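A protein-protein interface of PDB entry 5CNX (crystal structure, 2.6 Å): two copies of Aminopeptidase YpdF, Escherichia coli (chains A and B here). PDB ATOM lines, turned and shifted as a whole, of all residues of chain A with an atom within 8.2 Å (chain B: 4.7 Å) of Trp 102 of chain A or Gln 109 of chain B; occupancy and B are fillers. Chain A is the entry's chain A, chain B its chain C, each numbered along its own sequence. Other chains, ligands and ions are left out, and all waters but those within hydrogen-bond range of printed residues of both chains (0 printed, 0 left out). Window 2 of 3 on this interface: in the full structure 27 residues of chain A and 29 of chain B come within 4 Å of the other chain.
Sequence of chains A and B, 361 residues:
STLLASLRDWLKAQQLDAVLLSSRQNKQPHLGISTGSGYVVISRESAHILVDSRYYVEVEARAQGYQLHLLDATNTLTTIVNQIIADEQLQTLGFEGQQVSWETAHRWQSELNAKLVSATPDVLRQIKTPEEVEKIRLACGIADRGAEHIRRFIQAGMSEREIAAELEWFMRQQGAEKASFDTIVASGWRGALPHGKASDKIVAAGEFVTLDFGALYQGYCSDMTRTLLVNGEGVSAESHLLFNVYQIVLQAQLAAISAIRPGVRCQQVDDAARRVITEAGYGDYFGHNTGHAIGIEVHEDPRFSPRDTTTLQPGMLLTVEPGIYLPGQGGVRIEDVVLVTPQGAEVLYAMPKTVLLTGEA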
ATOM      1  N   PHE A  95      -5.031  14.716 -15.669  1.00  0.00           N
ATOM      2  CA  PHE A  95      -5.481  13.621 -14.822  1.00  0.00           C
ATOM      3  C   PHE A  95      -6.552  14.133 -13.887  1.00  0.00           C
ATOM      4  O   PHE A  95      -6.628  15.330 -13.622  1.00  0.00           O
ATOM      5  CB  PHE A  95      -4.331  13.015 -14.028  1.00  0.00           C
ATOM      6  CG  PHE A  95      -3.907  13.839 -12.844  1.00  0.00           C
ATOM      7  CD1 PHE A  95      -3.099  14.956 -13.013  1.00  0.00           C
ATOM      8  CD2 PHE A  95      -4.301  13.486 -11.555  1.00  0.00           C
ATOM      9  CE1 PHE A  95      -2.702  15.708 -11.936  1.00  0.00           C
ATOM     10  CE2 PHE A  95      -3.903  14.242 -10.465  1.00  0.00           C
ATOM     11  CZ  PHE A  95      -3.097  15.349 -10.659  1.00  0.00           C
ATOM     12  N   GLY A  97      -7.608  15.149 -10.891  1.00  0.00           N
ATOM     13  CA  GLY A  97      -7.093  15.560  -9.598  1.00  0.00           C
ATOM     14  C   GLY A  97      -8.105  15.505  -8.464  1.00  0.00           C
ATOM     15  O   GLY A  97      -7.724  15.582  -7.297  1.00  0.00           O
ATOM     16  N   GLN A  99     -10.151  12.895  -8.203  1.00  0.00           N
ATOM     17  CA  GLN A  99     -10.469  11.481  -8.056  1.00  0.00           C
ATOM     18  C   GLN A  99      -9.215  10.689  -7.680  1.00  0.00           C
ATOM     19  O   GLN A  99      -9.289   9.581  -7.156  1.00  0.00           O
ATOM     20  CB  GLN A  99     -11.066  10.934  -9.354  1.00  0.00           C
ATOM     21  CG  GLN A  99     -12.238  11.738  -9.890  1.00  0.00           C
ATOM     22  CD  GLN A  99     -13.482  11.603  -9.050  1.00  0.00           C
ATOM     23  OE1 GLN A  99     -13.673  10.604  -8.359  1.00  0.00           O
ATOM     24  NE2 GLN A  99     -14.348  12.599  -9.121  1.00  0.00           N
ATOM     25  N   VAL A 100      -8.056  11.251  -7.981  1.00  0.00           N
ATOM     26  CA  VAL A 100      -6.802  10.601  -7.662  1.00  0.00           C
ATOM     27  C   VAL A 100      -6.294  11.140  -6.327  1.00  0.00           C
ATOM     28  O   VAL A 100      -6.330  12.347  -6.076  1.00  0.00           O
ATOM     29  CB  VAL A 100      -5.781  10.827  -8.781  1.00  0.00           C
ATOM     30  CG1 VAL A 100      -4.457  10.219  -8.440  1.00  0.00           C
ATOM     31  CG2 VAL A 100      -6.314  10.255 -10.085  1.00  0.00           C
ATOM     32  N   SER A 101      -5.843  10.250  -5.456  1.00  0.00           N
ATOM     33  CA  SER A 101      -5.379  10.685  -4.141  1.00  0.00           C
ATOM     34  C   SER A 101      -4.108  11.521  -4.224  1.00  0.00           C
ATOM     35  O   SER A 101      -3.363  11.462  -5.215  1.00  0.00           O
ATOM     36  CB  SER A 101      -5.139   9.488  -3.212  1.00  0.00           C
ATOM     37  OG  SER A 101      -3.934   8.826  -3.539  1.00  0.00           O
ATOM     38  N   TRP A 102      -3.880  12.300  -3.177  1.00  0.00           N
ATOM     39  CA  TRP A 102      -2.671  13.080  -3.032  1.00  0.00           C
ATOM     40  C   TRP A 102      -1.434  12.221  -3.240  1.00  0.00           C
ATOM     41  O   TRP A 102      -0.534  12.596  -3.982  1.00  0.00           O
ATOM     42  CB  TRP A 102      -2.665  13.709  -1.640  1.00  0.00           C
ATOM     43  CG  TRP A 102      -1.368  14.320  -1.181  1.00  0.00           C
ATOM     44  CD1 TRP A 102      -0.421  13.725  -0.388  1.00  0.00           C
ATOM     45  CD2 TRP A 102      -0.892  15.645  -1.446  1.00  0.00           C
ATOM     46  NE1 TRP A 102       0.614  14.595  -0.156  1.00  0.00           N
ATOM     47  CE2 TRP A 102       0.354  15.780  -0.794  1.00  0.00           C
ATOM     48  CE3 TRP A 102      -1.392  16.727  -2.175  1.00  0.00           C
ATOM     49  CZ2 TRP A 102       1.104  16.955  -0.847  1.00  0.00           C
ATOM     50  CZ3 TRP A 102      -0.647  17.892  -2.227  1.00  0.00           C
ATOM     51  CH2 TRP A 102       0.590  17.997  -1.564  1.00  0.00           C
ATOM     52  N   GLU A 103      -1.411  11.047  -2.624  1.00  0.00           N
ATOM     53  CA  GLU A 103      -0.253  10.168  -2.720  1.00  0.00           C
ATOM     54  C   GLU A 103      -0.052   9.644  -4.138  1.00  0.00           C
ATOM     55  O   GLU A 103       1.062   9.639  -4.659  1.00  0.00           O
ATOM     56  CB  GLU A 103      -0.411   9.004  -1.752  1.00  0.00           C
ATOM     57  CG  GLU A 103      -0.207   9.409  -0.314  1.00  0.00           C
ATOM     58  CD  GLU A 103       1.211   9.193   0.151  1.00  0.00           C
ATOM     59  OE1 GLU A 103       1.793   8.135  -0.197  1.00  0.00           O
ATOM     60  OE2 GLU A 103       1.734  10.084   0.866  1.00  0.00           O
ATOM     61  N   THR A 104      -1.140   9.199  -4.755  1.00  0.00           N
ATOM     62  CA  THR A 104      -1.080   8.625  -6.094  1.00  0.00           C
ATOM     63  C   THR A 104      -0.664   9.642  -7.166  1.00  0.00           C
ATOM     64  O   THR A 104       0.142   9.333  -8.047  1.00  0.00           O
ATOM     65  CB  THR A 104      -2.423   8.011  -6.495  1.00  0.00           C
ATOM     66  OG1 THR A 104      -2.764   6.970  -5.573  1.00  0.00           O
ATOM     67  CG2 THR A 104      -2.339   7.434  -7.914  1.00  0.00           C
ATOM     68  N   ALA A 105      -1.216  10.846  -7.093  1.00  0.00           N
ATOM     69  CA  ALA A 105      -0.865  11.872  -8.061  1.00  0.00           C
ATOM     70  C   ALA A 105       0.614  12.211  -7.961  1.00  0.00           C
ATOM     71  O   ALA A 105       1.274  12.430  -8.977  1.00  0.00           O
ATOM     72  CB  ALA A 105      -1.714  13.108  -7.865  1.00  0.00           C
ATOM     73  N   HIS A 106       1.132  12.271  -6.738  1.00  0.00           N
ATOM     74  CA  HIS A 106       2.550  12.537  -6.542  1.00  0.00           C
ATOM     75  C   HIS A 106       3.417  11.460  -7.170  1.00  0.00           C
ATOM     76  O   HIS A 106       4.434  11.774  -7.791  1.00  0.00           O
ATOM     77  CB  HIS A 106       2.881  12.668  -5.064  1.00  0.00           C
ATOM     78  CG  HIS A 106       2.689  14.051  -4.527  1.00  0.00           C
ATOM     79  ND1 HIS A 106       3.711  14.971  -4.469  1.00  0.00           N
ATOM     80  CD2 HIS A 106       1.594  14.668  -4.023  1.00  0.00           C
ATOM     81  CE1 HIS A 106       3.253  16.099  -3.953  1.00  0.00           C
ATOM     82  NE2 HIS A 106       1.973  15.940  -3.674  1.00  0.00           N
ATOM     83  N   ARG A 107       3.018  10.197  -7.020  1.00  0.00           N
ATOM     84  CA  ARG A 107       3.770   9.095  -7.614  1.00  0.00           C
ATOM     85  C   ARG A 107       3.744   9.189  -9.140  1.00  0.00           C
ATOM     86  O   ARG A 107       4.769   9.036  -9.799  1.00  0.00           O
ATOM     87  CB  ARG A 107       3.199   7.738  -7.189  1.00  0.00           C
ATOM     88  CG  ARG A 107       3.986   6.562  -7.767  1.00  0.00           C
ATOM     89  CD  ARG A 107       3.489   5.193  -7.306  1.00  0.00           C
ATOM     90  NE  ARG A 107       2.137   4.902  -7.792  1.00  0.00           N
ATOM     91  CZ  ARG A 107       1.051   4.824  -7.028  1.00  0.00           C
ATOM     92  NH1 ARG A 107       1.140   5.018  -5.718  1.00  0.00           N
ATOM     93  NH2 ARG A 107      -0.127   4.545  -7.579  1.00  0.00           N
ATOM     94  N   TRP A 108       2.560   9.445  -9.689  1.00  0.00           N
ATOM     95  CA  TRP A 108       2.382   9.584 -11.134  1.00  0.00           C
ATOM     96  C   TRP A 108       3.211  10.713 -11.729  1.00  0.00           C
ATOM     97  O   TRP A 108       3.847  10.536 -12.767  1.00  0.00           O
ATOM     98  CB  TRP A 108       0.910   9.810 -11.484  1.00  0.00           C
ATOM     99  CG  TRP A 108       0.048   8.596 -11.337  1.00  0.00           C
ATOM    100  CD1 TRP A 108       0.445   7.348 -10.958  1.00  0.00           C
ATOM    101  CD2 TRP A 108      -1.355   8.510 -11.596  1.00  0.00           C
ATOM    102  NE1 TRP A 108      -0.628   6.495 -10.944  1.00  0.00           N
ATOM    103  CE2 TRP A 108      -1.746   7.181 -11.332  1.00  0.00           C
ATOM    104  CE3 TRP A 108      -2.323   9.429 -12.015  1.00  0.00           C
ATOM    105  CZ2 TRP A 108      -3.066   6.747 -11.474  1.00  0.00           C
ATOM    106  CZ3 TRP A 108      -3.631   9.000 -12.155  1.00  0.00           C
ATOM    107  CH2 TRP A 108      -3.993   7.672 -11.884  1.00  0.00           C
ATOM    108  N   GLN A 109       3.188  11.878 -11.086  1.00  0.00           N
ATOM    109  CA  GLN A 109       3.910  13.042 -11.594  1.00  0.00           C
ATOM    110  C   GLN A 109       5.402  12.763 -11.771  1.00  0.00           C
ATOM    111  O   GLN A 109       6.054  13.378 -12.612  1.00  0.00           O
ATOM    112  CB  GLN A 109       3.705  14.253 -10.675  1.00  0.00           C
ATOM    113  CG  GLN A 109       4.335  15.550 -11.188  1.00  0.00           C
ATOM    114  CD  GLN A 109       3.711  16.064 -12.486  1.00  0.00           C
ATOM    115  OE1 GLN A 109       4.070  15.625 -13.583  1.00  0.00           O
ATOM    116  NE2 GLN A 109       2.793  17.020 -12.365  1.00  0.00           N
ATOM    117  N   PHE B  95      -3.181  14.546   7.710  1.00  0.00           N
ATOM    118  CA  PHE B  95      -4.290  14.239   6.811  1.00  0.00           C
ATOM    119  C   PHE B  95      -4.074  12.914   6.073  1.00  0.00           C
ATOM    120  O   PHE B  95      -2.938  12.466   5.874  1.00  0.00           O
ATOM    121  CB  PHE B  95      -4.507  15.367   5.796  1.00  0.00           C
ATOM    122  CG  PHE B  95      -3.474  15.415   4.701  1.00  0.00           C
ATOM    123  CD1 PHE B  95      -2.238  16.012   4.918  1.00  0.00           C
ATOM    124  CD2 PHE B  95      -3.729  14.845   3.462  1.00  0.00           C
ATOM    125  CE1 PHE B  95      -1.287  16.051   3.914  1.00  0.00           C
ATOM    126  CE2 PHE B  95      -2.780  14.879   2.459  1.00  0.00           C
ATOM    127  CZ  PHE B  95      -1.561  15.483   2.681  1.00  0.00           C
ATOM    128  N   GLY B  97      -3.435  11.175   3.247  1.00  0.00           N
ATOM    129  CA  GLY B  97      -2.958  11.385   1.892  1.00  0.00           C
ATOM    130  C   GLY B  97      -3.318  10.311   0.876  1.00  0.00           C
ATOM    131  O   GLY B  97      -3.157  10.513  -0.331  1.00  0.00           O
ATOM    132  N   VAL B 100      -7.506  11.396   0.518  1.00  0.00           N
ATOM    133  CA  VAL B 100      -7.869  12.732   0.064  1.00  0.00           C
ATOM    134  C   VAL B 100      -7.383  12.952  -1.365  1.00  0.00           C
ATOM    135  O   VAL B 100      -6.267  12.562  -1.710  1.00  0.00           O
ATOM    136  CB  VAL B 100      -7.277  13.806   0.979  1.00  0.00           C
ATOM    137  CG1 VAL B 100      -7.650  15.191   0.501  1.00  0.00           C
ATOM    138  CG2 VAL B 100      -7.766  13.598   2.385  1.00  0.00           C
ATOM    139  N   SER B 101      -8.227  13.547  -2.207  1.00  0.00           N
ATOM    140  CA  SER B 101      -7.842  13.791  -3.598  1.00  0.00           C
ATOM    141  C   SER B 101      -6.698  14.797  -3.653  1.00  0.00           C
ATOM    142  O   SER B 101      -6.526  15.613  -2.735  1.00  0.00           O
ATOM    143  CB  SER B 101      -9.030  14.293  -4.425  1.00  0.00           C
ATOM    144  OG  SER B 101      -9.326  15.649  -4.149  1.00  0.00           O
ATOM    145  N   TRP B 102      -5.919  14.736  -4.727  1.00  0.00           N
ATOM    146  CA  TRP B 102      -4.803  15.651  -4.893  1.00  0.00           C
ATOM    147  C   TRP B 102      -5.312  17.086  -4.768  1.00  0.00           C
ATOM    148  O   TRP B 102      -4.678  17.938  -4.141  1.00  0.00           O
ATOM    149  CB  TRP B 102      -4.088  15.432  -6.225  1.00  0.00           C
ATOM    150  CG  TRP B 102      -3.014  16.434  -6.429  1.00  0.00           C
ATOM    151  CD1 TRP B 102      -1.712  16.321  -6.037  1.00  0.00           C
ATOM    152  CD2 TRP B 102      -3.146  17.724  -7.031  1.00  0.00           C
ATOM    153  NE1 TRP B 102      -1.020  17.458  -6.370  1.00  0.00           N
ATOM    154  CE2 TRP B 102      -1.876  18.335  -6.982  1.00  0.00           C
ATOM    155  CE3 TRP B 102      -4.210  18.420  -7.609  1.00  0.00           C
ATOM    156  CZ2 TRP B 102      -1.646  19.610  -7.494  1.00  0.00           C
ATOM    157  CZ3 TRP B 102      -3.983  19.679  -8.109  1.00  0.00           C
ATOM    158  CH2 TRP B 102      -2.710  20.265  -8.050  1.00  0.00           C
ATOM    159  N   ALA B 105      -6.304  18.045  -0.998  1.00  0.00           N
ATOM    160  CA  ALA B 105      -5.114  18.190  -0.173  1.00  0.00           C
ATOM    161  C   ALA B 105      -4.378  19.456  -0.578  1.00  0.00           C
ATOM    162  O   ALA B 105      -3.920  20.215   0.273  1.00  0.00           O
ATOM    163  CB  ALA B 105      -4.209  16.970  -0.302  1.00  0.00           C
ATOM    164  N   HIS B 106      -4.316  19.691  -1.884  1.00  0.00           N
ATOM    165  CA  HIS B 106      -3.655  20.861  -2.441  1.00  0.00           C
ATOM    166  C   HIS B 106      -4.298  22.172  -1.975  1.00  0.00           C
ATOM    167  O   HIS B 106      -3.580  23.105  -1.643  1.00  0.00           O
ATOM    168  CB  HIS B 106      -3.639  20.752  -3.971  1.00  0.00           C
ATOM    169  CG  HIS B 106      -2.969  21.896  -4.663  1.00  0.00           C
ATOM    170  ND1 HIS B 106      -1.618  22.139  -4.557  1.00  0.00           N
ATOM    171  CD2 HIS B 106      -3.467  22.855  -5.481  1.00  0.00           C
ATOM    172  CE1 HIS B 106      -1.311  23.211  -5.273  1.00  0.00           C
ATOM    173  NE2 HIS B 106      -2.413  23.663  -5.841  1.00  0.00           N
ATOM    174  N   ARG B 107      -5.628  22.247  -1.933  1.00  0.00           N
ATOM    175  CA  ARG B 107      -6.299  23.452  -1.419  1.00  0.00           C
ATOM    176  C   ARG B 107      -5.979  23.627   0.072  1.00  0.00           C
ATOM    177  O   ARG B 107      -5.730  24.738   0.530  1.00  0.00           O
ATOM    178  CB  ARG B 107      -7.827  23.407  -1.636  1.00  0.00           C
ATOM    179  CG  ARG B 107      -8.567  22.514  -0.643  1.00  0.00           C
ATOM    180  CD  ARG B 107     -10.082  22.499  -0.718  1.00  0.00           C
ATOM    181  NE  ARG B 107     -10.612  22.007  -1.987  1.00  0.00           N
ATOM    182  CZ  ARG B 107     -11.339  22.761  -2.804  1.00  0.00           C
ATOM    183  NH1 ARG B 107     -11.599  24.022  -2.465  1.00  0.00           N
ATOM    184  NH2 ARG B 107     -11.803  22.264  -3.947  1.00  0.00           N
ATOM    185  N   TRP B 108      -6.012  22.516   0.813  1.00  0.00           N
ATOM    186  CA  TRP B 108      -5.706  22.488   2.239  1.00  0.00           C
ATOM    187  C   TRP B 108      -4.294  22.981   2.452  1.00  0.00           C
ATOM    188  O   TRP B 108      -4.042  23.863   3.272  1.00  0.00           O
ATOM    189  CB  TRP B 108      -5.844  21.071   2.796  1.00  0.00           C
ATOM    190  CG  TRP B 108      -7.240  20.569   2.930  1.00  0.00           C
ATOM    191  CD1 TRP B 108      -8.392  21.258   2.678  1.00  0.00           C
ATOM    192  CD2 TRP B 108      -7.640  19.242   3.310  1.00  0.00           C
ATOM    193  NE1 TRP B 108      -9.483  20.447   2.893  1.00  0.00           N
ATOM    194  CE2 TRP B 108      -9.049  19.207   3.287  1.00  0.00           C
ATOM    195  CE3 TRP B 108      -6.943  18.086   3.686  1.00  0.00           C
ATOM    196  CZ2 TRP B 108      -9.776  18.063   3.626  1.00  0.00           C
ATOM    197  CZ3 TRP B 108      -7.667  16.946   4.014  1.00  0.00           C
ATOM    198  CH2 TRP B 108      -9.067  16.944   3.980  1.00  0.00           C
ATOM    199  N   GLN B 109      -3.395  22.438   1.640  1.00  0.00           N
ATOM    200  CA  GLN B 109      -1.974  22.709   1.725  1.00  0.00           C
ATOM    201  C   GLN B 109      -1.720  24.213   1.647  1.00  0.00           C
ATOM    202  O   GLN B 109      -0.723  24.715   2.162  1.00  0.00           O
ATOM    203  CB  GLN B 109      -1.249  21.968   0.604  1.00  0.00           C
ATOM    204  CG  GLN B 109       0.243  21.999   0.700  1.00  0.00           C
ATOM    205  CD  GLN B 109       0.727  21.256   1.930  1.00  0.00           C
ATOM    206  OE1 GLN B 109       0.791  21.818   3.033  1.00  0.00           O
ATOM    207  NE2 GLN B 109       1.034  19.970   1.758  1.00  0.00           N
ATOM    208  N   SER B 110      -2.635  24.926   0.998  1.00  0.00           N
ATOM    209  CA  SER B 110      -2.531  26.371   0.865  1.00  0.00           C
ATOM    210  C   SER B 110      -3.432  27.136   1.845  1.00  0.00           C
ATOM    211  O   SER B 110      -3.097  28.240   2.251  1.00  0.00           O
ATOM    212  CB  SER B 110      -2.848  26.789  -0.581  1.00  0.00           C
ATOM    213  OG  SER B 110      -4.241  26.778  -0.844  1.00  0.00           O
ATOM    214  N   GLU B 111      -4.589  26.575   2.187  1.00  0.00           N
ATOM    215  CA  GLU B 111      -5.559  27.275   3.036  1.00  0.00           C
ATOM    216  C   GLU B 111      -5.440  27.032   4.548  1.00  0.00           C
ATOM    217  O   GLU B 111      -5.999  27.792   5.342  1.00  0.00           O
ATOM    218  CB  GLU B 111      -6.982  26.935   2.599  1.00  0.00           C
ATOM    219  CG  GLU B 111      -7.325  27.421   1.210  1.00  0.00           C
ATOM    220  CD  GLU B 111      -8.807  27.341   0.919  1.00  0.00           C
ATOM    221  OE1 GLU B 111      -9.528  26.652   1.675  1.00  0.00           O
ATOM    222  OE2 GLU B 111      -9.250  27.978  -0.061  1.00  0.00           O
ATOM    223  N   LEU B 116       0.920  20.726   6.901  1.00  0.00           N
ATOM    224  CA  LEU B 116       0.159  19.528   6.595  1.00  0.00           C
ATOM    225  C   LEU B 116       1.065  18.361   6.229  1.00  0.00           C
ATOM    226  O   LEU B 116       1.952  18.485   5.381  1.00  0.00           O
ATOM    227  CB  LEU B 116      -0.833  19.819   5.471  1.00  0.00           C
ATOM    228  CG  LEU B 116      -2.213  20.270   5.960  1.00  0.00           C
ATOM    229  CD1 LEU B 116      -2.155  21.552   6.775  1.00  0.00           C
ATOM    230  CD2 LEU B 116      -3.131  20.466   4.784  1.00  0.00           C
ATOM    231  N   SER B 118       1.072  14.108   5.305  1.00  0.00           N
ATOM    232  CA  SER B 118       0.331  12.917   4.922  1.00  0.00           C
ATOM    233  C   SER B 118       0.647  11.756   5.867  1.00  0.00           C
ATOM    234  O   SER B 118       1.760  11.213   5.862  1.00  0.00           O
ATOM    235  CB  SER B 118       0.645  12.538   3.477  1.00  0.00           C
ATOM    236  OG  SER B 118      -0.073  11.383   3.086  1.00  0.00           O
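The backbone carbonyl oxygen of Gly 97 of chain A is in hydrogen-bond range of the backbone NH of Trp 102 of chain B (3.3 Å). O of Val 100 of chain A is in hydrogen-bond range of N of Trp 102 of chain B (2.8 Å). O of Gly 97 of chain B lies within hydrogen-bond range of N of Trp 102 of chain A, at 3.4 Å. N of Trp 102 of chain A is in hydrogen-bond range of O of Val 100 of chain B (2.8 Å). The backbone carbonyl oxygen of Gly 97 of chain B lies within hydrogen-bond range of the backbone NH of Glu 103 of chain A (2.9 Å). The side-chain hydroxyl (OG) of Ser 118 of chain B sits at hydrogen-bond distance from the side-chain carboxylate (OE2) of Glu 103 of chain A (3.1 Å).
The side-chain hydroxyl (OG) of Ser 101 of chain A lies close to the backbone NH (N) of Glu 103 of chain A (3.5 Å). The side-chain hydroxyl (OG) of Ser 101 of chain A sits at hydrogen-bond distance from the side-chain hydroxyl (OG1) of Thr 104 of chain A (3.0 Å). The side-chain hydroxyl (OG) of Ser 118 of chain B lies close to the backbone NH (N) of Gly 97 of chain B.
O of Gly 97 of chain A touches CB of Ser 101 of chain B, at 3.4 Å. CA of Ser 101 of chain B touches O of Val 100 of chain A, 3.2 Å away. Ser 101 of chain A touches Val 100 of chain B (CA to O, 3.2 Å). Ser 101 of chain A touches Trp 102 of chain B. NE1 of Trp 102 of chain A touches CZ of Phe 95 of chain B (3.7 Å). Ser 101 of chain B touches Trp 102 of chain A. Trp 102 of chain B touches Trp 102 of chain A. Trp 102 of chain A touches Ala 105 of chain B. Trp 102 of chain A touches Gln 109 of chain B. Trp 102 of chain B touches Ala 105 of chain A.
Of the printed residues of chain B, Gly 97 of chain A touches Ser 101 (3.4 Å) and Trp 102 (3.3 Å). Printed residues of chain B within 4 Å of Val 100 of chain A: Ser 101 and Trp 102. Trp 102 of chain A touches just these residues of chain B: Phe 95 (3.7 Å), Gly 97 (3.4 Å), Val 100 (2.8 Å), Ser 101 (3.8 Å), Trp 102 (3.5 Å), Ala 105 (3.4 Å) and Gln 109 (3.9 Å). Thr 104 of chain A touches none of the printed residues of chain B. Of the printed residues of chain B, Ala 105 of chain A touches Trp 102 (3.7 Å). Gln 109 of chain A touches none of the printed residues of chain B. Of the printed residues of chain A, Phe 95 of chain B touches Trp 102 (3.7 Å). Printed residues of chain A within 4 Å of Val 100 of chain B: Ser 101 and Trp 102. Of chain A, only Trp 102 (3.9 Å) comes within 4 Å of Gln 109 of chain B.
Of the 13 printed residues of chain A, 6 touch a printed residue of chain B. Of the 14 printed residues of chain B, 8 touch a printed residue of chain A. Printed residues of chain B that touch a printed residue of chain A: Phe 95, Gly 97, Val 100, Ser 101, Trp 102, Ala 105, Gln 109 and Ser 118. Among the printed residues, 17 pairs touch across the chains.
Gly 97 of chain A touches Ser 101 of chain B, and with the chains exchanged Ser 101 of chain A touches Gly 97 of chain B. Trp 102 of chain A touches Phe 95 of chain B, but with the chains exchanged Phe 95 of chain A does not touch Trp 102 of chain B (4.3 Å). Trp 102 of chain B touches its own counterpart, Trp 102 of chain A. Trp 102 of chain A touches Ala 105 of chain B, and with the chains exchanged Ala 105 of chain A touches Trp 102 of chain B. 10 positions are printed for both chains. Of the 17 pairs that touch across the chains among the printed residues, 13 have their exchanged pair printed and touching as well.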
